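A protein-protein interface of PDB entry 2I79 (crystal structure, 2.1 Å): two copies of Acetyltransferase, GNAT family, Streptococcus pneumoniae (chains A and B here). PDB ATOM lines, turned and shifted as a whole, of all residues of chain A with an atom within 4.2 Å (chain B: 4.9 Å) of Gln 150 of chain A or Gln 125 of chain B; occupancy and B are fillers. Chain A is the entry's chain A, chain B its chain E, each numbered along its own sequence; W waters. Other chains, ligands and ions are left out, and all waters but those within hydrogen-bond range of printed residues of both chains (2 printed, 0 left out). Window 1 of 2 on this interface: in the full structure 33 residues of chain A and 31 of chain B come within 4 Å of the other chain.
The backbone NH of Ser 149 of chain A is in hydrogen-bond range of the backbone carbonyl oxygen of Glu 147 of chain B.
The side-chain amide nitrogen (NE2) of Gln 150 of chain A sits close to the guanidinium group (NH2) of Arg 123 of chain B, 3.2 Å away.
The side-chain amide nitrogen (NE2) of Gln 150 of chain A is in hydrogen-bond range of the side-chain carboxylate (OE1) of Glu 147 of chain B (3.3 Å).
The backbone carbonyl oxygen (O) of Glu 151 of chain A is in hydrogen-bond range of the guanidinium group (NH1) of Arg 123 of chain B (2.9 Å).
The backbone carbonyl oxygen (O) of Arg 123 of chain B lies within hydrogen-bond range of the backbone NH (N) of Gly 88 of chain B (2.9 Å).
N of Gln 125 of chain B is in hydrogen-bond range of O of Gly 88 of chain B.
The side-chain amide nitrogen (NE2) of Gln 125 of chain B lies within hydrogen-bond range of the side-chain carboxylate (OD1) of Asp 89 of chain B (2.7 Å).
The guanidinium group (NE) of Arg 123 of chain B lies within hydrogen-bond range of the side-chain amide oxygen (OE1) of Gln 125 of chain B.
O of Leu 166 of chain B lies within hydrogen-bond range of N of Glu 147 of chain B, at 2.7 Å.
The side-chain carboxylate (OE1) of Glu 147 of chain B is in hydrogen-bond range of the backbone NH (N) of Gly 168 of chain B (3.3 Å).
Gln 125 of chain B touches Gln 150 of chain A.
Leu 166 of chain B touches Gln 150 of chain A (CB to NE2, 3.7 Å).
Ile 87 of chain B touches Arg 152 of chain A.
Arg 152 of chain A touches Arg 123 of chain B (O to CD, 3.5 Å).
Ile 87 of chain B touches Gly 153 of chain A (CD1 to O, 3.4 Å).
Leu 166 of chain A touches Leu 166 of chain B (CD1 to CD1, 3.4 Å).
Of the printed residues of chain B, Gln 150 of chain A touches Arg 123, Gln 125, Glu 147 and Leu 166.
Of the printed residues of chain B, Glu 151 of chain A touches Arg 123 (2.9 Å).
Of the printed residues of chain B, Leu 166 of chain A touches Leu 166.
Of the printed residues of chain A, Arg 123 of chain B touches Gln 150 (3.2 Å), Glu 151 (2.9 Å) and Arg 152 (3.5 Å).
Printed residues of chain A within 4 Å of Gln 125 of chain B: Gln 150.
Leu 126 of chain B touches none of the printed residues of chain A.
Of the printed residues of chain A, Leu 166 of chain B touches Gln 150 (3.7 Å) and Leu 166 (3.4 Å).
The nearest printed residue of chain B that does not touch Gln 150 of chain A is Met 167 of chain B (4.9 Å).
The nearest printed residue of chain A that does not touch Gln 125 of chain B is Gly 153 of chain A (6.1 Å).
The nearest printed residue of chain A that does not touch Glu 147 of chain B is Leu 166 of chain A (4.3 Å).
Printed residues of chain B that touch a printed residue of chain A: Ile 87, Arg 123, Gln 125, Glu 147 and Leu 166.
Hydrophobic or aromatic side chains of chain B within 4 Å of the printed part of chain A: Ile 87 and Leu 166.
Along chain B the printed residues that touch a printed residue of chain A span positions 87 to 166.
Among the printed residues, 10 pairs touch across the chains.
Among the printed residues, no Asp or Glu carboxylate lies within 4 Å of a Lys or Arg side-chain nitrogen of the other chain.
Leu 166 of chain A touches its own counterpart, Leu 166 of chain B.
Of the 10 pairs that touch across the chains among the printed residues, 1 has its exchanged pair printed and touching as well.
Water W1 lies within hydrogen-bond range of OE2 of Glu 147 of chain B (2.5 Å) and N of Glu 151 of chain A (2.9 Å).
Water W2 lies within hydrogen-bond range of OE1 of Gln 150 of chain A and OE1 of Gln 125 of chain B.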
ATOM      1  N   SER A 149       6.947   2.524  -1.718  1.00  0.00           N
ATOM      2  CA  SER A 149       5.745   2.134  -1.001  1.00  0.00           C
ATOM      3  C   SER A 149       6.123   1.277   0.185  1.00  0.00           C
ATOM      4  O   SER A 149       7.185   0.613   0.178  1.00  0.00           O
ATOM      5  CB  SER A 149       4.747   1.419  -1.917  1.00  0.00           C
ATOM      6  OG  SER A 149       5.157   0.110  -2.187  1.00  0.00           O
ATOM      7  N   GLN A 150       5.282   1.361   1.222  1.00  0.00           N
ATOM      8  CA  GLN A 150       5.568   0.800   2.536  1.00  0.00           C
ATOM      9  C   GLN A 150       4.349   0.004   3.026  1.00  0.00           C
ATOM     10  O   GLN A 150       3.223   0.501   3.148  1.00  0.00           O
ATOM     11  CB  GLN A 150       5.992   1.906   3.532  1.00  0.00           C
ATOM     12  CG  GLN A 150       7.372   2.503   3.166  1.00  0.00           C
ATOM     13  CD  GLN A 150       7.849   3.601   4.058  1.00  0.00           C
ATOM     14  OE1 GLN A 150       7.066   4.387   4.547  1.00  0.00           O
ATOM     15  NE2 GLN A 150       9.157   3.667   4.276  1.00  0.00           N
ATOM     16  N   GLU A 151       4.605  -1.265   3.266  1.00  0.00           N
ATOM     17  CA  GLU A 151       3.622  -2.165   3.826  1.00  0.00           C
ATOM     18  C   GLU A 151       3.434  -1.868   5.345  1.00  0.00           C
ATOM     19  O   GLU A 151       4.381  -1.612   6.045  1.00  0.00           O
ATOM     20  CB  GLU A 151       4.096  -3.585   3.562  1.00  0.00           C
ATOM     21  CG  GLU A 151       3.008  -4.598   3.619  1.00  0.00           C
ATOM     22  CD  GLU A 151       3.489  -6.007   3.191  1.00  0.00           C
ATOM     23  OE1 GLU A 151       2.822  -6.995   3.586  1.00  0.00           O
ATOM     24  OE2 GLU A 151       4.543  -6.103   2.506  1.00  0.00           O
ATOM     25  N   ARG A 152       2.187  -1.900   5.803  1.00  0.00           N
ATOM     26  CA  ARG A 152       1.788  -1.488   7.129  1.00  0.00           C
ATOM     27  C   ARG A 152       2.108  -0.020   7.390  1.00  0.00           C
ATOM     28  O   ARG A 152       2.409   0.344   8.500  1.00  0.00           O
ATOM     29  CB  ARG A 152       2.430  -2.371   8.212  1.00  0.00           C
ATOM     30  CG  ARG A 152       2.287  -3.848   7.946  1.00  0.00           C
ATOM     31  CD  ARG A 152       2.775  -4.684   9.067  1.00  0.00           C
ATOM     32  NE  ARG A 152       2.451  -6.086   8.806  1.00  0.00           N
ATOM     33  CZ  ARG A 152       2.853  -7.128   9.533  1.00  0.00           C
ATOM     34  NH1 ARG A 152       3.639  -6.975  10.588  1.00  0.00           N
ATOM     35  NH2 ARG A 152       2.482  -8.355   9.175  1.00  0.00           N
ATOM     36  N   GLY A 153       2.056   0.825   6.375  1.00  0.00           N
ATOM     37  CA  GLY A 153       2.225   2.251   6.572  1.00  0.00           C
ATOM     38  C   GLY A 153       1.113   2.874   7.409  1.00  0.00           C
ATOM     39  O   GLY A 153       1.285   3.936   7.995  1.00  0.00           O
ATOM     40  N   ASP A 163      -1.051  -0.346   2.866  1.00  0.00           N
ATOM     41  CA  ASP A 163       0.144   0.266   2.291  1.00  0.00           C
ATOM     42  C   ASP A 163      -0.016   1.759   2.041  1.00  0.00           C
ATOM     43  O   ASP A 163      -1.120   2.269   1.775  1.00  0.00           O
ATOM     44  CB  ASP A 163       0.509  -0.375   0.931  1.00  0.00           C
ATOM     45  CG  ASP A 163       0.966  -1.839   1.043  1.00  0.00           C
ATOM     46  OD1 ASP A 163       0.381  -2.618   1.806  1.00  0.00           O
ATOM     47  OD2 ASP A 163       1.914  -2.227   0.334  1.00  0.00           O
ATOM     48  N   VAL A 164       1.131   2.427   2.057  1.00  0.00           N
ATOM     49  CA  VAL A 164       1.271   3.835   1.696  1.00  0.00           C
ATOM     50  C   VAL A 164       2.295   4.027   0.569  1.00  0.00           C
ATOM     51  O   VAL A 164       3.236   3.271   0.447  1.00  0.00           O
ATOM     52  CB  VAL A 164       1.642   4.706   2.909  1.00  0.00           C
ATOM     53  CG1 VAL A 164       0.536   4.620   3.963  1.00  0.00           C
ATOM     54  CG2 VAL A 164       3.025   4.343   3.536  1.00  0.00           C
ATOM     55  N   LEU A 166       5.187   6.595  -0.706  1.00  0.00           N
ATOM     56  CA  LEU A 166       6.073   7.736  -0.508  1.00  0.00           C
ATOM     57  C   LEU A 166       6.049   8.609  -1.760  1.00  0.00           C
ATOM     58  O   LEU A 166       6.304   8.102  -2.869  1.00  0.00           O
ATOM     59  CB  LEU A 166       7.503   7.211  -0.357  1.00  0.00           C
ATOM     60  CG  LEU A 166       7.811   6.205   0.748  1.00  0.00           C
ATOM     61  CD1 LEU A 166       9.193   5.549   0.446  1.00  0.00           C
ATOM     62  CD2 LEU A 166       7.780   6.946   2.078  1.00  0.00           C
ATOM     63  N   ILE B  87       4.292   1.553  14.317  1.00  0.00           N
ATOM     64  CA  ILE B  87       5.514   1.812  13.545  1.00  0.00           C
ATOM     65  C   ILE B  87       6.594   2.432  14.440  1.00  0.00           C
ATOM     66  O   ILE B  87       6.426   3.530  14.990  1.00  0.00           O
ATOM     67  CB  ILE B  87       5.254   2.755  12.334  1.00  0.00           C
ATOM     68  CG1 ILE B  87       3.999   2.315  11.585  1.00  0.00           C
ATOM     69  CG2 ILE B  87       6.498   2.825  11.434  1.00  0.00           C
ATOM     70  CD1 ILE B  87       3.678   3.127  10.323  1.00  0.00           C
ATOM     71  N   GLY B  88       7.712   1.724  14.554  1.00  0.00           N
ATOM     72  CA  GLY B  88       8.890   2.250  15.196  1.00  0.00           C
ATOM     73  C   GLY B  88       9.935   2.750  14.223  1.00  0.00           C
ATOM     74  O   GLY B  88      10.338   2.020  13.329  1.00  0.00           O
ATOM     75  N   ASP B  89      10.368   4.006  14.408  1.00  0.00           N
ATOM     76  CA  ASP B  89      11.446   4.615  13.640  1.00  0.00           C
ATOM     77  C   ASP B  89      12.755   4.331  14.343  1.00  0.00           C
ATOM     78  O   ASP B  89      12.897   4.604  15.529  1.00  0.00           O
ATOM     79  CB  ASP B  89      11.247   6.113  13.527  1.00  0.00           C
ATOM     80  CG  ASP B  89      10.014   6.463  12.751  1.00  0.00           C
ATOM     81  OD1 ASP B  89       9.995   6.221  11.518  1.00  0.00           O
ATOM     82  OD2 ASP B  89       9.056   6.975  13.372  1.00  0.00           O
ATOM     83  N   LEU B  90      13.707   3.779  13.612  1.00  0.00           N
ATOM     84  CA  LEU B  90      14.952   3.307  14.200  1.00  0.00           C
ATOM     85  C   LEU B  90      16.104   4.264  13.990  1.00  0.00           C
ATOM     86  O   LEU B  90      16.202   4.946  12.956  1.00  0.00           O
ATOM     87  CB  LEU B  90      15.315   1.947  13.605  1.00  0.00           C
ATOM     88  CG  LEU B  90      14.780   0.774  14.424  1.00  0.00           C
ATOM     89  CD1 LEU B  90      14.150  -0.215  13.530  1.00  0.00           C
ATOM     90  CD2 LEU B  90      15.887   0.157  15.274  1.00  0.00           C
ATOM     91  N   ARG B 123       5.947  -2.849  12.639  1.00  0.00           N
ATOM     92  CA  ARG B 123       6.793  -2.375  11.583  1.00  0.00           C
ATOM     93  C   ARG B 123       7.927  -1.571  12.186  1.00  0.00           C
ATOM     94  O   ARG B 123       7.751  -0.808  13.137  1.00  0.00           O
ATOM     95  CB  ARG B 123       5.974  -1.540  10.596  1.00  0.00           C
ATOM     96  CG  ARG B 123       6.778  -0.883   9.535  1.00  0.00           C
ATOM     97  CD  ARG B 123       5.912  -0.046   8.590  1.00  0.00           C
ATOM     98  NE  ARG B 123       6.820   0.786   7.805  1.00  0.00           N
ATOM     99  CZ  ARG B 123       7.431   0.403   6.690  1.00  0.00           C
ATOM    100  NH1 ARG B 123       7.169  -0.772   6.125  1.00  0.00           N
ATOM    101  NH2 ARG B 123       8.289   1.228   6.119  1.00  0.00           N
ATOM    102  N   LEU B 124       9.123  -1.815  11.662  1.00  0.00           N
ATOM    103  CA  LEU B 124      10.290  -1.024  11.973  1.00  0.00           C
ATOM    104  C   LEU B 124      10.796  -0.377  10.682  1.00  0.00           C
ATOM    105  O   LEU B 124      10.759  -1.000   9.619  1.00  0.00           O
ATOM    106  CB  LEU B 124      11.365  -1.907  12.579  1.00  0.00           C
ATOM    107  CG  LEU B 124      11.156  -2.379  14.017  1.00  0.00           C
ATOM    108  CD1 LEU B 124      12.401  -3.187  14.433  1.00  0.00           C
ATOM    109  CD2 LEU B 124      10.848  -1.230  14.972  1.00  0.00           C
ATOM    110  N   GLN B 125      11.283   0.860  10.772  1.00  0.00           N
ATOM    111  CA  GLN B 125      11.648   1.606   9.560  1.00  0.00           C
ATOM    112  C   GLN B 125      12.706   2.673   9.818  1.00  0.00           C
ATOM    113  O   GLN B 125      12.899   3.145  10.966  1.00  0.00           O
ATOM    114  CB  GLN B 125      10.396   2.273   8.936  1.00  0.00           C
ATOM    115  CG  GLN B 125       9.833   3.444   9.757  1.00  0.00           C
ATOM    116  CD  GLN B 125       8.603   4.071   9.148  1.00  0.00           C
ATOM    117  OE1 GLN B 125       7.923   3.461   8.332  1.00  0.00           O
ATOM    118  NE2 GLN B 125       8.293   5.297   9.566  1.00  0.00           N
ATOM    119  N   LEU B 126      13.345   3.092   8.733  1.00  0.00           N
ATOM    120  CA  LEU B 126      14.314   4.169   8.757  1.00  0.00           C
ATOM    121  C   LEU B 126      14.661   4.708   7.384  1.00  0.00           C
ATOM    122  O   LEU B 126      14.309   4.110   6.360  1.00  0.00           O
ATOM    123  CB  LEU B 126      15.595   3.752   9.483  1.00  0.00           C
ATOM    124  CG  LEU B 126      16.603   2.819   8.840  1.00  0.00           C
ATOM    125  CD1 LEU B 126      17.910   3.074   9.584  1.00  0.00           C
ATOM    126  CD2 LEU B 126      16.232   1.353   8.914  1.00  0.00           C
ATOM    127  N   THR B 127      15.382   5.826   7.383  1.00  0.00           N
ATOM    128  CA  THR B 127      15.925   6.448   6.177  1.00  0.00           C
ATOM    129  C   THR B 127      17.443   6.362   6.272  1.00  0.00           C
ATOM    130  O   THR B 127      18.020   6.662   7.319  1.00  0.00           O
ATOM    131  CB  THR B 127      15.489   7.917   6.065  1.00  0.00           C
ATOM    132  OG1 THR B 127      14.074   7.955   5.908  1.00  0.00           O
ATOM    133  CG2 THR B 127      16.074   8.582   4.836  1.00  0.00           C
ATOM    134  N   PHE B 144      15.864  -5.979   6.890  1.00  0.00           N
ATOM    135  CA  PHE B 144      15.281  -4.755   6.334  1.00  0.00           C
ATOM    136  C   PHE B 144      15.425  -4.774   4.809  1.00  0.00           C
ATOM    137  O   PHE B 144      16.466  -5.133   4.290  1.00  0.00           O
ATOM    138  CB  PHE B 144      15.927  -3.477   6.918  1.00  0.00           C
ATOM    139  CG  PHE B 144      15.518  -3.178   8.335  1.00  0.00           C
ATOM    140  CD1 PHE B 144      14.701  -2.112   8.622  1.00  0.00           C
ATOM    141  CD2 PHE B 144      15.950  -3.965   9.380  1.00  0.00           C
ATOM    142  CE1 PHE B 144      14.336  -1.831   9.914  1.00  0.00           C
ATOM    143  CE2 PHE B 144      15.583  -3.697  10.653  1.00  0.00           C
ATOM    144  CZ  PHE B 144      14.777  -2.632  10.921  1.00  0.00           C
ATOM    145  N   GLU B 147      12.652   0.102   0.395  1.00  0.00           N
ATOM    146  CA  GLU B 147      11.252   0.343  -0.001  1.00  0.00           C
ATOM    147  C   GLU B 147      11.060   1.563  -0.889  1.00  0.00           C
ATOM    148  O   GLU B 147      10.003   1.755  -1.469  1.00  0.00           O
ATOM    149  CB  GLU B 147      10.390   0.516   1.249  1.00  0.00           C
ATOM    150  CG  GLU B 147      10.201  -0.782   1.984  1.00  0.00           C
ATOM    151  CD  GLU B 147       9.646  -0.607   3.369  1.00  0.00           C
ATOM    152  OE1 GLU B 147       9.911   0.441   3.998  1.00  0.00           O
ATOM    153  OE2 GLU B 147       8.942  -1.536   3.823  1.00  0.00           O
ATOM    154  N   LEU B 166      14.675   4.431   1.766  1.00  0.00           N
ATOM    155  CA  LEU B 166      13.841   4.067   2.897  1.00  0.00           C
ATOM    156  C   LEU B 166      13.835   2.561   3.051  1.00  0.00           C
ATOM    157  O   LEU B 166      13.806   1.831   2.059  1.00  0.00           O
ATOM    158  CB  LEU B 166      12.420   4.590   2.718  1.00  0.00           C
ATOM    159  CG  LEU B 166      12.476   6.113   2.665  1.00  0.00           C
ATOM    160  CD1 LEU B 166      12.406   6.473   1.164  1.00  0.00           C
ATOM    161  CD2 LEU B 166      11.365   6.742   3.446  1.00  0.00           C
ATOM    162  N   MET B 167      13.856   2.120   4.303  1.00  0.00           N
ATOM    163  CA  MET B 167      14.007   0.706   4.634  1.00  0.00           C
ATOM    164  C   MET B 167      13.021   0.374   5.722  1.00  0.00           C
ATOM    165  O   MET B 167      12.827   1.166   6.646  1.00  0.00           O
ATOM    166  CB  MET B 167      15.436   0.362   5.093  1.00  0.00           C
ATOM    167  CG  MET B 167      16.555   0.718   4.077  1.00  0.00           C
ATOM    168  SD  MET B 167      18.222   0.093   4.459  1.00  0.00           S
ATOM    169  CE  MET B 167      17.970  -1.654   4.147  1.00  0.00           C
ATOM    170  N   GLY B 168      12.445  -0.815   5.634  1.00  0.00           N
ATOM    171  CA  GLY B 168      11.516  -1.300   6.631  1.00  0.00           C
ATOM    172  C   GLY B 168      11.603  -2.794   6.848  1.00  0.00           C
ATOM    173  O   GLY B 168      12.142  -3.523   6.020  1.00  0.00           O
HETATM  174  O   HOH W   1       7.054  -2.493   2.431  1.00  0.00           O
HETATM  175  O   HOH W   2       5.567   4.170   6.684  1.00  0.00           O
